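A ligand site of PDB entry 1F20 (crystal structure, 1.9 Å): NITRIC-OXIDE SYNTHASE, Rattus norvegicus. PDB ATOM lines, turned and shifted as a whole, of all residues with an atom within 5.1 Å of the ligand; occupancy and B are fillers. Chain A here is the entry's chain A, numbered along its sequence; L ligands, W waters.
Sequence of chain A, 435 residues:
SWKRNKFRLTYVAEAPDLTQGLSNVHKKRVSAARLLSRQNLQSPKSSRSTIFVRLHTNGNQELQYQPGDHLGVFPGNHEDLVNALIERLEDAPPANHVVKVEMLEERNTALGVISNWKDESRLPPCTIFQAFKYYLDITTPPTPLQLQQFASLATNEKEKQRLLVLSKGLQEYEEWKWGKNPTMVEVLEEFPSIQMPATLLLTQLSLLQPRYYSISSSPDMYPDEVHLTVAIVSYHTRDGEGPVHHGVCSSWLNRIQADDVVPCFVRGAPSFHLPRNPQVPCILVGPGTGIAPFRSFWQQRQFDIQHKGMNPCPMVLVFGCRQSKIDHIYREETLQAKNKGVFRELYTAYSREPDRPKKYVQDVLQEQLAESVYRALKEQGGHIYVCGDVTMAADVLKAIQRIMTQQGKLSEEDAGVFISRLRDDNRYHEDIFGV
The guanidinium group (NE) of Arg 211 is in salt-bridge range of an oxygen (O13) of the ligand (2.9 Å).
The backbone carbonyl oxygen of Thr 229 lies within hydrogen-bond range of a nitrogen (N7) of the ligand (2.6 Å).
An oxygen (O8) of the ligand is in hydrogen-bond range of the backbone NH (N) of Ser 214 (2.9 Å).
N of Val 248 is in hydrogen-bond range of O2 of the ligand, 2.8 Å away.
The backbone NH of Ala 231 sits at hydrogen-bond distance from an oxygen (O7) of the ligand, at 2.8 Å.
An oxygen (O11) of the ligand lies within hydrogen-bond range of the side-chain hydroxyl (OH) of Tyr 213.
The backbone NH of Cys 249 lies within hydrogen-bond range of an oxygen (O13) of the ligand, at 2.7 Å.
OG of Ser 250 is in hydrogen-bond range of O14 of the ligand (2.9 Å).
An oxygen (O9) of the ligand lies within hydrogen-bond range of the backbone carbonyl oxygen of Tyr 212 (2.7 Å).
N of Tyr 212 is in hydrogen-bond range of O9 of the ligand.
The backbone NH (N) of Ser 250 lies within hydrogen-bond range of an oxygen (O14) of the ligand (2.9 Å).
The backbone NH (N) of Val 233 sits at hydrogen-bond distance from the side-chain hydroxyl (OG) of Ser 250 (3.2 Å).
N of Arg 267 is in hydrogen-bond range of O of His 70 (2.9 Å).
NE2 of His 70 sits at hydrogen-bond distance from OD1 of Asp 431.
OH of Tyr 235 sits at hydrogen-bond distance from OD1 of Asn 181 (2.6 Å).
The side-chain hydroxyl (OG) of Ser 251 sits at hydrogen-bond distance from the backbone carbonyl oxygen (O) of Gly 247 (2.6 Å).
OG of Ser 214 sits at hydrogen-bond distance from OD2 of Asp 431.
The backbone carbonyl oxygen of Val 233 lies within hydrogen-bond range of the backbone NH of Gly 247, 2.8 Å away.
O of Val 248 sits at hydrogen-bond distance from OG of Ser 251, 3.1 Å away.
Merely in contact with the ligand: His 70 (3.5 Å), Val 230 (3.5 Å), Val 233 (3.5 Å), Tyr 235 (3.2 Å), Gly 247 (3.3 Å), Arg 267 (3.3 Å), Thr 289 (3.3 Å), Ala 292 (3.8 Å), Phe 433 (3.3 Å) and Gly 434 (3.7 Å).
Hydrophobic or aromatic side chains within 4 Å of the ligand: His 70, Tyr 212, Tyr 213, Ala 231, Val 233, Tyr 235, Val 248, Ala 292 and Phe 433.
Within 4 Å of the ligand: His 70, Arg 211, Tyr 212, Tyr 213, Ser 214, Thr 229, Val 230, Ala 231, Val 233, Tyr 235, Gly 247, Val 248, Cys 249, Ser 250, Arg 267, Thr 289, Ala 292, Phe 433 and Gly 434.
Along chain A the residues within 4 Å of the ligand span positions 70 to 434.
Water W12 bridges O11 of the ligand (2.6 Å) and O of Ala 231 (2.8 Å).
Water W11 bridges an oxygen (O9) of the ligand (2.7 Å) and the backbone NH (N) of Tyr 212 (3.0 Å).
Water W7 lies within hydrogen-bond range of the backbone carbonyl oxygen (O) of Ser 214, the backbone NH (N) of Thr 229 and an oxygen (O8) of the ligand.
Water W9 lies within hydrogen-bond range of O of Gly 434 (2.5 Å), O10 of the ligand (2.9 Å) and O of Val 435 (3.5 Å).
Water W2 lies within hydrogen-bond range of the backbone carbonyl oxygen of His 246 (2.8 Å), an oxygen (O2) of the ligand (3.3 Å) and the side-chain hydroxyl of Thr 139 (3.4 Å).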
ATOM      1  N   HIS A  70     -11.910   2.291   0.347  1.00  0.00           N
ATOM      2  CA  HIS A  70     -10.682   1.871   0.999  1.00  0.00           C
ATOM      3  C   HIS A  70     -10.879   1.783   2.503  1.00  0.00           C
ATOM      4  O   HIS A  70     -11.808   2.383   3.056  1.00  0.00           O
ATOM      5  CB  HIS A  70      -9.551   2.873   0.741  1.00  0.00           C
ATOM      6  CG  HIS A  70      -9.154   2.978  -0.691  1.00  0.00           C
ATOM      7  ND1 HIS A  70      -9.427   4.092  -1.463  1.00  0.00           N
ATOM      8  CD2 HIS A  70      -8.497   2.108  -1.503  1.00  0.00           C
ATOM      9  CE1 HIS A  70      -8.946   3.896  -2.679  1.00  0.00           C
ATOM     10  NE2 HIS A  70      -8.380   2.708  -2.727  1.00  0.00           N
ATOM     11  N   THR A 139      10.450   3.286  12.426  1.00  0.00           N
ATOM     12  CA  THR A 139      11.082   2.544  11.350  1.00  0.00           C
ATOM     13  C   THR A 139      11.741   3.413  10.256  1.00  0.00           C
ATOM     14  O   THR A 139      12.764   3.039   9.699  1.00  0.00           O
ATOM     15  CB  THR A 139      10.013   1.633  10.740  1.00  0.00           C
ATOM     16  OG1 THR A 139      10.615   0.534  10.042  1.00  0.00           O
ATOM     17  CG2 THR A 139       9.211   2.425   9.804  1.00  0.00           C
ATOM     18  N   ASN A 181      18.886   1.226   5.133  1.00  0.00           N
ATOM     19  CA  ASN A 181      17.471   1.464   5.422  1.00  0.00           C
ATOM     20  C   ASN A 181      17.288   1.277   6.935  1.00  0.00           C
ATOM     21  O   ASN A 181      16.382   0.591   7.385  1.00  0.00           O
ATOM     22  CB  ASN A 181      16.632   0.441   4.636  1.00  0.00           C
ATOM     23  CG  ASN A 181      15.159   0.461   5.017  1.00  0.00           C
ATOM     24  OD1 ASN A 181      14.605  -0.561   5.422  1.00  0.00           O
ATOM     25  ND2 ASN A 181      14.520   1.615   4.868  1.00  0.00           N
ATOM     26  N   ARG A 211      -2.438   2.772   7.031  1.00  0.00           N
ATOM     27  CA  ARG A 211      -2.163   2.295   5.686  1.00  0.00           C
ATOM     28  C   ARG A 211      -3.513   1.992   5.032  1.00  0.00           C
ATOM     29  O   ARG A 211      -4.395   1.418   5.662  1.00  0.00           O
ATOM     30  CB  ARG A 211      -1.320   1.016   5.711  1.00  0.00           C
ATOM     31  CG  ARG A 211       0.179   1.260   5.738  1.00  0.00           C
ATOM     32  CD  ARG A 211       0.664   1.861   7.055  1.00  0.00           C
ATOM     33  NE  ARG A 211       2.124   1.767   7.133  1.00  0.00           N
ATOM     34  CZ  ARG A 211       2.896   2.460   7.964  1.00  0.00           C
ATOM     35  NH1 ARG A 211       2.363   3.317   8.825  1.00  0.00           N
ATOM     36  NH2 ARG A 211       4.204   2.297   7.921  1.00  0.00           N
ATOM     37  N   TYR A 212      -3.658   2.370   3.762  1.00  0.00           N
ATOM     38  CA  TYR A 212      -4.899   2.139   3.039  1.00  0.00           C
ATOM     39  C   TYR A 212      -4.900   0.844   2.242  1.00  0.00           C
ATOM     40  O   TYR A 212      -3.881   0.442   1.669  1.00  0.00           O
ATOM     41  CB  TYR A 212      -5.169   3.330   2.102  1.00  0.00           C
ATOM     42  CG  TYR A 212      -5.485   4.599   2.865  1.00  0.00           C
ATOM     43  CD1 TYR A 212      -6.762   4.823   3.379  1.00  0.00           C
ATOM     44  CD2 TYR A 212      -4.489   5.531   3.148  1.00  0.00           C
ATOM     45  CE1 TYR A 212      -7.037   5.941   4.156  1.00  0.00           C
ATOM     46  CE2 TYR A 212      -4.751   6.655   3.920  1.00  0.00           C
ATOM     47  CZ  TYR A 212      -6.028   6.864   4.420  1.00  0.00           C
ATOM     48  OH  TYR A 212      -6.288   7.964   5.200  1.00  0.00           O
ATOM     49  N   TYR A 213      -6.055   0.183   2.204  1.00  0.00           N
ATOM     50  CA  TYR A 213      -6.206  -1.071   1.469  1.00  0.00           C
ATOM     51  C   TYR A 213      -7.549  -1.055   0.743  1.00  0.00           C
ATOM     52  O   TYR A 213      -8.544  -0.592   1.286  1.00  0.00           O
ATOM     53  CB  TYR A 213      -6.141  -2.255   2.434  1.00  0.00           C
ATOM     54  CG  TYR A 213      -4.776  -2.372   3.077  1.00  0.00           C
ATOM     55  CD1 TYR A 213      -3.726  -3.002   2.412  1.00  0.00           C
ATOM     56  CD2 TYR A 213      -4.504  -1.770   4.304  1.00  0.00           C
ATOM     57  CE1 TYR A 213      -2.442  -3.033   2.952  1.00  0.00           C
ATOM     58  CE2 TYR A 213      -3.230  -1.784   4.857  1.00  0.00           C
ATOM     59  CZ  TYR A 213      -2.196  -2.416   4.167  1.00  0.00           C
ATOM     60  OH  TYR A 213      -0.922  -2.421   4.684  1.00  0.00           O
ATOM     61  N   SER A 214      -7.559  -1.556  -0.491  1.00  0.00           N
ATOM     62  CA  SER A 214      -8.789  -1.595  -1.267  1.00  0.00           C
ATOM     63  C   SER A 214      -9.671  -2.724  -0.754  1.00  0.00           C
ATOM     64  O   SER A 214      -9.290  -3.893  -0.799  1.00  0.00           O
ATOM     65  CB  SER A 214      -8.489  -1.806  -2.746  1.00  0.00           C
ATOM     66  OG  SER A 214      -7.729  -0.721  -3.243  1.00  0.00           O
ATOM     67  N   THR A 229      -6.859  -7.641   0.646  1.00  0.00           N
ATOM     68  CA  THR A 229      -5.893  -8.425  -0.119  1.00  0.00           C
ATOM     69  C   THR A 229      -4.579  -7.675   0.129  1.00  0.00           C
ATOM     70  O   THR A 229      -4.418  -6.535  -0.316  1.00  0.00           O
ATOM     71  CB  THR A 229      -6.236  -8.412  -1.620  1.00  0.00           C
ATOM     72  OG1 THR A 229      -7.577  -8.884  -1.783  1.00  0.00           O
ATOM     73  CG2 THR A 229      -5.292  -9.335  -2.407  1.00  0.00           C
ATOM     74  N   VAL A 230      -3.668  -8.311   0.853  1.00  0.00           N
ATOM     75  CA  VAL A 230      -2.418  -7.649   1.238  1.00  0.00           C
ATOM     76  C   VAL A 230      -1.126  -8.322   0.820  1.00  0.00           C
ATOM     77  O   VAL A 230      -0.870  -9.475   1.183  1.00  0.00           O
ATOM     78  CB  VAL A 230      -2.390  -7.467   2.774  1.00  0.00           C
ATOM     79  CG1 VAL A 230      -1.170  -6.647   3.206  1.00  0.00           C
ATOM     80  CG2 VAL A 230      -3.702  -6.829   3.237  1.00  0.00           C
ATOM     81  N   ALA A 231      -0.310  -7.590   0.062  1.00  0.00           N
ATOM     82  CA  ALA A 231       0.982  -8.093  -0.388  1.00  0.00           C
ATOM     83  C   ALA A 231       1.904  -7.962   0.814  1.00  0.00           C
ATOM     84  O   ALA A 231       1.948  -6.914   1.442  1.00  0.00           O
ATOM     85  CB  ALA A 231       1.495  -7.240  -1.558  1.00  0.00           C
ATOM     86  N   VAL A 233       5.192  -7.214   2.513  1.00  0.00           N
ATOM     87  CA  VAL A 233       6.421  -6.498   2.228  1.00  0.00           C
ATOM     88  C   VAL A 233       7.544  -6.926   3.161  1.00  0.00           C
ATOM     89  O   VAL A 233       7.432  -6.766   4.384  1.00  0.00           O
ATOM     90  CB  VAL A 233       6.214  -4.976   2.354  1.00  0.00           C
ATOM     91  CG1 VAL A 233       7.529  -4.249   2.124  1.00  0.00           C
ATOM     92  CG2 VAL A 233       5.163  -4.519   1.365  1.00  0.00           C
ATOM     93  N   TYR A 235      12.088  -7.314   2.987  1.00  0.00           N
ATOM     94  CA  TYR A 235      13.270  -7.104   2.177  1.00  0.00           C
ATOM     95  C   TYR A 235      14.611  -7.206   2.902  1.00  0.00           C
ATOM     96  O   TYR A 235      14.727  -6.868   4.077  1.00  0.00           O
ATOM     97  CB  TYR A 235      13.191  -5.733   1.517  1.00  0.00           C
ATOM     98  CG  TYR A 235      12.934  -4.603   2.471  1.00  0.00           C
ATOM     99  CD1 TYR A 235      11.630  -4.251   2.830  1.00  0.00           C
ATOM    100  CD2 TYR A 235      13.988  -3.849   2.996  1.00  0.00           C
ATOM    101  CE1 TYR A 235      11.380  -3.174   3.684  1.00  0.00           C
ATOM    102  CE2 TYR A 235      13.748  -2.774   3.852  1.00  0.00           C
ATOM    103  CZ  TYR A 235      12.441  -2.444   4.202  1.00  0.00           C
ATOM    104  OH  TYR A 235      12.184  -1.377   5.025  1.00  0.00           O
ATOM    105  N   HIS A 246      10.677  -5.735   7.490  1.00  0.00           N
ATOM    106  CA  HIS A 246       9.312  -6.016   7.087  1.00  0.00           C
ATOM    107  C   HIS A 246       8.450  -4.759   7.122  1.00  0.00           C
ATOM    108  O   HIS A 246       8.609  -3.905   8.004  1.00  0.00           O
ATOM    109  CB  HIS A 246       8.710  -7.064   8.031  1.00  0.00           C
ATOM    110  CG  HIS A 246       9.457  -8.367   8.027  1.00  0.00           C
ATOM    111  ND1 HIS A 246       9.415  -9.238   6.969  1.00  0.00           N
ATOM    112  CD2 HIS A 246      10.283  -8.923   8.951  1.00  0.00           C
ATOM    113  CE1 HIS A 246      10.175 -10.286   7.233  1.00  0.00           C
ATOM    114  NE2 HIS A 246      10.718 -10.116   8.425  1.00  0.00           N
ATOM    115  N   GLY A 247       7.543  -4.647   6.159  1.00  0.00           N
ATOM    116  CA  GLY A 247       6.639  -3.521   6.126  1.00  0.00           C
ATOM    117  C   GLY A 247       5.881  -3.569   7.436  1.00  0.00           C
ATOM    118  O   GLY A 247       5.472  -4.639   7.894  1.00  0.00           O
ATOM    119  N   VAL A 248       5.690  -2.410   8.065  1.00  0.00           N
ATOM    120  CA  VAL A 248       4.997  -2.361   9.341  1.00  0.00           C
ATOM    121  C   VAL A 248       3.573  -2.927   9.347  1.00  0.00           C
ATOM    122  O   VAL A 248       3.278  -3.870  10.077  1.00  0.00           O
ATOM    123  CB  VAL A 248       4.965  -0.915   9.894  1.00  0.00           C
ATOM    124  CG1 VAL A 248       4.168  -0.842  11.191  1.00  0.00           C
ATOM    125  CG2 VAL A 248       6.396  -0.436  10.141  1.00  0.00           C
ATOM    126  N   CYS A 249       2.686  -2.349   8.540  1.00  0.00           N
ATOM    127  CA  CYS A 249       1.299  -2.798   8.520  1.00  0.00           C
ATOM    128  C   CYS A 249       1.089  -4.177   7.901  1.00  0.00           C
ATOM    129  O   CYS A 249       0.333  -4.981   8.440  1.00  0.00           O
ATOM    130  CB  CYS A 249       0.413  -1.781   7.816  1.00  0.00           C
ATOM    131  SG  CYS A 249      -1.357  -2.004   8.143  1.00  0.00           S
ATOM    132  N   SER A 250       1.746  -4.469   6.780  1.00  0.00           N
ATOM    133  CA  SER A 250       1.554  -5.773   6.174  1.00  0.00           C
ATOM    134  C   SER A 250       2.047  -6.895   7.095  1.00  0.00           C
ATOM    135  O   SER A 250       1.389  -7.929   7.231  1.00  0.00           O
ATOM    136  CB  SER A 250       2.220  -5.851   4.790  1.00  0.00           C
ATOM    137  OG  SER A 250       3.634  -5.757   4.876  1.00  0.00           O
ATOM    138  N   SER A 251       3.188  -6.700   7.745  1.00  0.00           N
ATOM    139  CA  SER A 251       3.703  -7.730   8.636  1.00  0.00           C
ATOM    140  C   SER A 251       2.800  -7.860   9.878  1.00  0.00           C
ATOM    141  O   SER A 251       2.603  -8.959  10.395  1.00  0.00           O
ATOM    142  CB  SER A 251       5.144  -7.434   9.050  1.00  0.00           C
ATOM    143  OG  SER A 251       5.228  -6.262   9.848  1.00  0.00           O
ATOM    144  N   ARG A 267     -12.630   5.009   4.050  1.00  0.00           N
ATOM    145  CA  ARG A 267     -12.433   6.241   3.303  1.00  0.00           C
ATOM    146  C   ARG A 267     -13.090   5.995   1.954  1.00  0.00           C
ATOM    147  O   ARG A 267     -12.605   5.198   1.149  1.00  0.00           O
ATOM    148  CB  ARG A 267     -10.947   6.558   3.089  1.00  0.00           C
ATOM    149  CG  ARG A 267     -10.732   7.953   2.464  1.00  0.00           C
ATOM    150  CD  ARG A 267      -9.279   8.246   2.178  1.00  0.00           C
ATOM    151  NE  ARG A 267      -8.760   7.454   1.069  1.00  0.00           N
ATOM    152  CZ  ARG A 267      -7.493   7.451   0.679  1.00  0.00           C
ATOM    153  NH1 ARG A 267      -6.598   8.208   1.314  1.00  0.00           N
ATOM    154  NH2 ARG A 267      -7.117   6.705  -0.344  1.00  0.00           N
ATOM    155  N   THR A 289      -1.938  -7.600  -6.793  1.00  0.00           N
ATOM    156  CA  THR A 289      -2.830  -7.163  -5.728  1.00  0.00           C
ATOM    157  C   THR A 289      -3.830  -6.133  -6.225  1.00  0.00           C
ATOM    158  O   THR A 289      -4.789  -5.806  -5.531  1.00  0.00           O
ATOM    159  CB  THR A 289      -1.997  -6.598  -4.552  1.00  0.00           C
ATOM    160  OG1 THR A 289      -0.968  -7.543  -4.228  1.00  0.00           O
ATOM    161  CG2 THR A 289      -2.870  -6.391  -3.321  1.00  0.00           C
ATOM    162  N   ALA A 292      -7.644  -6.457  -5.969  1.00  0.00           N
ATOM    163  CA  ALA A 292      -8.357  -6.190  -4.716  1.00  0.00           C
ATOM    164  C   ALA A 292      -9.757  -5.556  -4.786  1.00  0.00           C
ATOM    165  O   ALA A 292     -10.734  -6.164  -4.351  1.00  0.00           O
ATOM    166  CB  ALA A 292      -7.454  -5.361  -3.782  1.00  0.00           C
ATOM    167  N   ASP A 431      -7.234   3.436  -9.247  1.00  0.00           N
ATOM    168  CA  ASP A 431      -7.028   3.171  -7.824  1.00  0.00           C
ATOM    169  C   ASP A 431      -5.539   2.812  -7.723  1.00  0.00           C
ATOM    170  O   ASP A 431      -5.178   1.638  -7.736  1.00  0.00           O
ATOM    171  CB  ASP A 431      -7.902   1.979  -7.376  1.00  0.00           C
ATOM    172  CG  ASP A 431      -7.868   1.736  -5.860  1.00  0.00           C
ATOM    173  OD1 ASP A 431      -7.098   2.409  -5.145  1.00  0.00           O
ATOM    174  OD2 ASP A 431      -8.614   0.846  -5.379  1.00  0.00           O
ATOM    175  N   ILE A 432      -4.680   3.816  -7.649  1.00  0.00           N
ATOM    176  CA  ILE A 432      -3.246   3.570  -7.594  1.00  0.00           C
ATOM    177  C   ILE A 432      -2.684   3.353  -6.186  1.00  0.00           C
ATOM    178  O   ILE A 432      -2.895   4.177  -5.292  1.00  0.00           O
ATOM    179  CB  ILE A 432      -2.470   4.723  -8.274  1.00  0.00           C
ATOM    180  CG1 ILE A 432      -2.883   4.811  -9.745  1.00  0.00           C
ATOM    181  CG2 ILE A 432      -0.975   4.509  -8.169  1.00  0.00           C
ATOM    182  CD1 ILE A 432      -2.282   5.983 -10.478  1.00  0.00           C
ATOM    183  N   PHE A 433      -1.968   2.249  -5.991  1.00  0.00           N
ATOM    184  CA  PHE A 433      -1.373   1.908  -4.701  1.00  0.00           C
ATOM    185  C   PHE A 433      -0.056   2.663  -4.510  1.00  0.00           C
ATOM    186  O   PHE A 433       1.011   2.088  -4.685  1.00  0.00           O
ATOM    187  CB  PHE A 433      -1.103   0.399  -4.610  1.00  0.00           C
ATOM    188  CG  PHE A 433      -2.354  -0.450  -4.636  1.00  0.00           C
ATOM    189  CD1 PHE A 433      -3.619   0.134  -4.707  1.00  0.00           C
ATOM    190  CD2 PHE A 433      -2.256  -1.847  -4.587  1.00  0.00           C
ATOM    191  CE1 PHE A 433      -4.773  -0.660  -4.718  1.00  0.00           C
ATOM    192  CE2 PHE A 433      -3.407  -2.634  -4.606  1.00  0.00           C
ATOM    193  CZ  PHE A 433      -4.672  -2.043  -4.669  1.00  0.00           C
ATOM    194  N   GLY A 434      -0.129   3.935  -4.136  1.00  0.00           N
ATOM    195  CA  GLY A 434       1.096   4.691  -3.958  1.00  0.00           C
ATOM    196  C   GLY A 434       1.923   4.427  -2.718  1.00  0.00           C
ATOM    197  O   GLY A 434       1.430   3.852  -1.734  1.00  0.00           O
ATOM    198  N   VAL A 435       3.176   4.878  -2.763  1.00  0.00           N
ATOM    199  CA  VAL A 435       4.115   4.726  -1.656  1.00  0.00           C
ATOM    200  C   VAL A 435       3.713   5.647  -0.534  1.00  0.00           C
ATOM    201  O   VAL A 435       2.740   6.380  -0.748  1.00  0.00           O
ATOM    202  CB  VAL A 435       5.574   5.093  -2.077  1.00  0.00           C
ATOM    203  CG1 VAL A 435       6.012   4.231  -3.241  1.00  0.00           C
ATOM    204  CG2 VAL A 435       5.633   6.589  -2.437  1.00  0.00           C
ATOM    205  OXT VAL A 435       4.369   5.623   0.521  1.00  0.00           O
HETATM  206  P1  LIG L   1       5.938   0.102   5.237  1.00  0.00           P
HETATM  207  O1  LIG L   1       5.291   1.390   5.197  1.00  0.00           O
HETATM  208  O2  LIG L   1       6.516  -0.176   6.538  1.00  0.00           O
HETATM  209  O3  LIG L   1       7.048   0.099   4.299  1.00  0.00           O
HETATM  210  C1  LIG L   1       6.752   0.307   2.877  1.00  0.00           C
HETATM  211  C2  LIG L   1       8.079   0.900   2.417  1.00  0.00           C
HETATM  212  O4  LIG L   1       8.981  -0.246   2.536  1.00  0.00           O
HETATM  213  C3  LIG L   1       8.216   1.214   0.939  1.00  0.00           C
HETATM  214  O5  LIG L   1       7.476   2.290   0.419  1.00  0.00           O
HETATM  215  C4  LIG L   1       9.689   1.369   0.872  1.00  0.00           C
HETATM  216  O6  LIG L   1      10.211   2.590   1.368  1.00  0.00           O
HETATM  217  C5  LIG L   1      10.149   0.164   1.748  1.00  0.00           C
HETATM  218  N1  LIG L   1      10.476  -1.051   1.003  1.00  0.00           N
HETATM  219  C6  LIG L   1       9.801  -2.178   0.454  1.00  0.00           C
HETATM  220  N2  LIG L   1      10.599  -3.046  -0.176  1.00  0.00           N
HETATM  221  C7  LIG L   1      11.866  -2.493  -0.057  1.00  0.00           C
HETATM  222  C8  LIG L   1      13.255  -2.931  -0.529  1.00  0.00           C
HETATM  223  N3  LIG L   1      13.462  -4.025  -1.204  1.00  0.00           N
HETATM  224  N4  LIG L   1      14.384  -2.052  -0.188  1.00  0.00           N
HETATM  225  C9  LIG L   1      14.240  -0.832   0.546  1.00  0.00           C
HETATM  226  N5  LIG L   1      12.997  -0.365   1.014  1.00  0.00           N
HETATM  227  C10 LIG L   1      11.838  -1.224   0.696  1.00  0.00           C
HETATM  228  N6  LIG L   1      -1.376  -2.736  -0.675  1.00  0.00           N
HETATM  229  C11 LIG L   1      -1.845  -4.005  -0.683  1.00  0.00           C
HETATM  230  O7  LIG L   1      -1.127  -4.936  -0.470  1.00  0.00           O
HETATM  231  N7  LIG L   1      -3.308  -4.220  -0.941  1.00  0.00           N
HETATM  232  C12 LIG L   1      -4.222  -3.112  -1.201  1.00  0.00           C
HETATM  233  O8  LIG L   1      -5.408  -3.313  -1.398  1.00  0.00           O
HETATM  234  C13 LIG L   1      -3.680  -1.742  -1.205  1.00  0.00           C
HETATM  235  N8  LIG L   1      -4.473  -0.631  -1.431  1.00  0.00           N
HETATM  236  C14 LIG L   1      -3.967   0.695  -1.422  1.00  0.00           C
HETATM  237  C15 LIG L   1      -4.889   1.826  -1.662  1.00  0.00           C
HETATM  238  C16 LIG L   1      -4.394   3.235  -1.647  1.00  0.00           C
HETATM  239  C17 LIG L   1      -5.393   4.350  -1.896  1.00  0.00           C
HETATM  240  C18 LIG L   1      -2.873   3.505  -1.347  1.00  0.00           C
HETATM  241  C19 LIG L   1      -2.223   4.893  -1.290  1.00  0.00           C
HETATM  242  C20 LIG L   1      -1.978   2.395  -1.098  1.00  0.00           C
HETATM  243  C21 LIG L   1      -2.474   0.979  -1.121  1.00  0.00           C
HETATM  244  N9  LIG L   1      -1.633  -0.249  -0.871  1.00  0.00           N
HETATM  245  C22 LIG L   1      -2.180  -1.598  -0.912  1.00  0.00           C
HETATM  246  C23 LIG L   1      -0.361  -0.220  -0.101  1.00  0.00           C
HETATM  247  C24 LIG L   1      -0.543  -0.102   1.446  1.00  0.00           C
HETATM  248  O9  LIG L   1      -1.243   1.058   1.834  1.00  0.00           O
HETATM  249  C25 LIG L   1       0.794  -0.082   2.194  1.00  0.00           C
HETATM  250  O10 LIG L   1       1.524   1.082   1.642  1.00  0.00           O
HETATM  251  C26 LIG L   1       1.702  -1.335   1.952  1.00  0.00           C
HETATM  252  O11 LIG L   1       0.914  -2.409   2.493  1.00  0.00           O
HETATM  253  C27 LIG L   1       3.049  -1.327   2.738  1.00  0.00           C
HETATM  254  O12 LIG L   1       2.816  -0.973   4.126  1.00  0.00           O
HETATM  255  P2  LIG L   1       3.697  -1.451   5.193  1.00  0.00           P
HETATM  256  O13 LIG L   1       3.223  -0.772   6.389  1.00  0.00           O
HETATM  257  O14 LIG L   1       3.569  -2.899   5.242  1.00  0.00           O
HETATM  258  O15 LIG L   1       5.022  -0.974   4.744  1.00  0.00           O
HETATM  259  O   HOH W   1       6.969  -2.701  -1.316  1.00  0.00           O
HETATM  260  O   HOH W   2       9.529  -1.328   7.364  1.00  0.00           O
HETATM  261  O   HOH W   3       3.321   2.306   3.350  1.00  0.00           O
HETATM  262  O   HOH W   4      17.632  -2.169  -0.836  1.00  0.00           O
HETATM  263  O   HOH W   5       6.387   4.123   5.518  1.00  0.00           O
HETATM  264  O   HOH W   6       5.056  -0.947  -0.090  1.00  0.00           O
HETATM  265  O   HOH W   7      -6.974  -4.962   0.123  1.00  0.00           O
HETATM  266  O   HOH W   8       3.593   1.055  -0.752  1.00  0.00           O
HETATM  267  O   HOH W   9       0.981   3.775   0.714  1.00  0.00           O
HETATM  268  O   HOH W  10       1.253  -2.197  -2.641  1.00  0.00           O
HETATM  269  O   HOH W  11      -1.262   3.686   2.489  1.00  0.00           O
HETATM  270  O   HOH W  12       1.096  -4.353   0.806  1.00  0.00           O
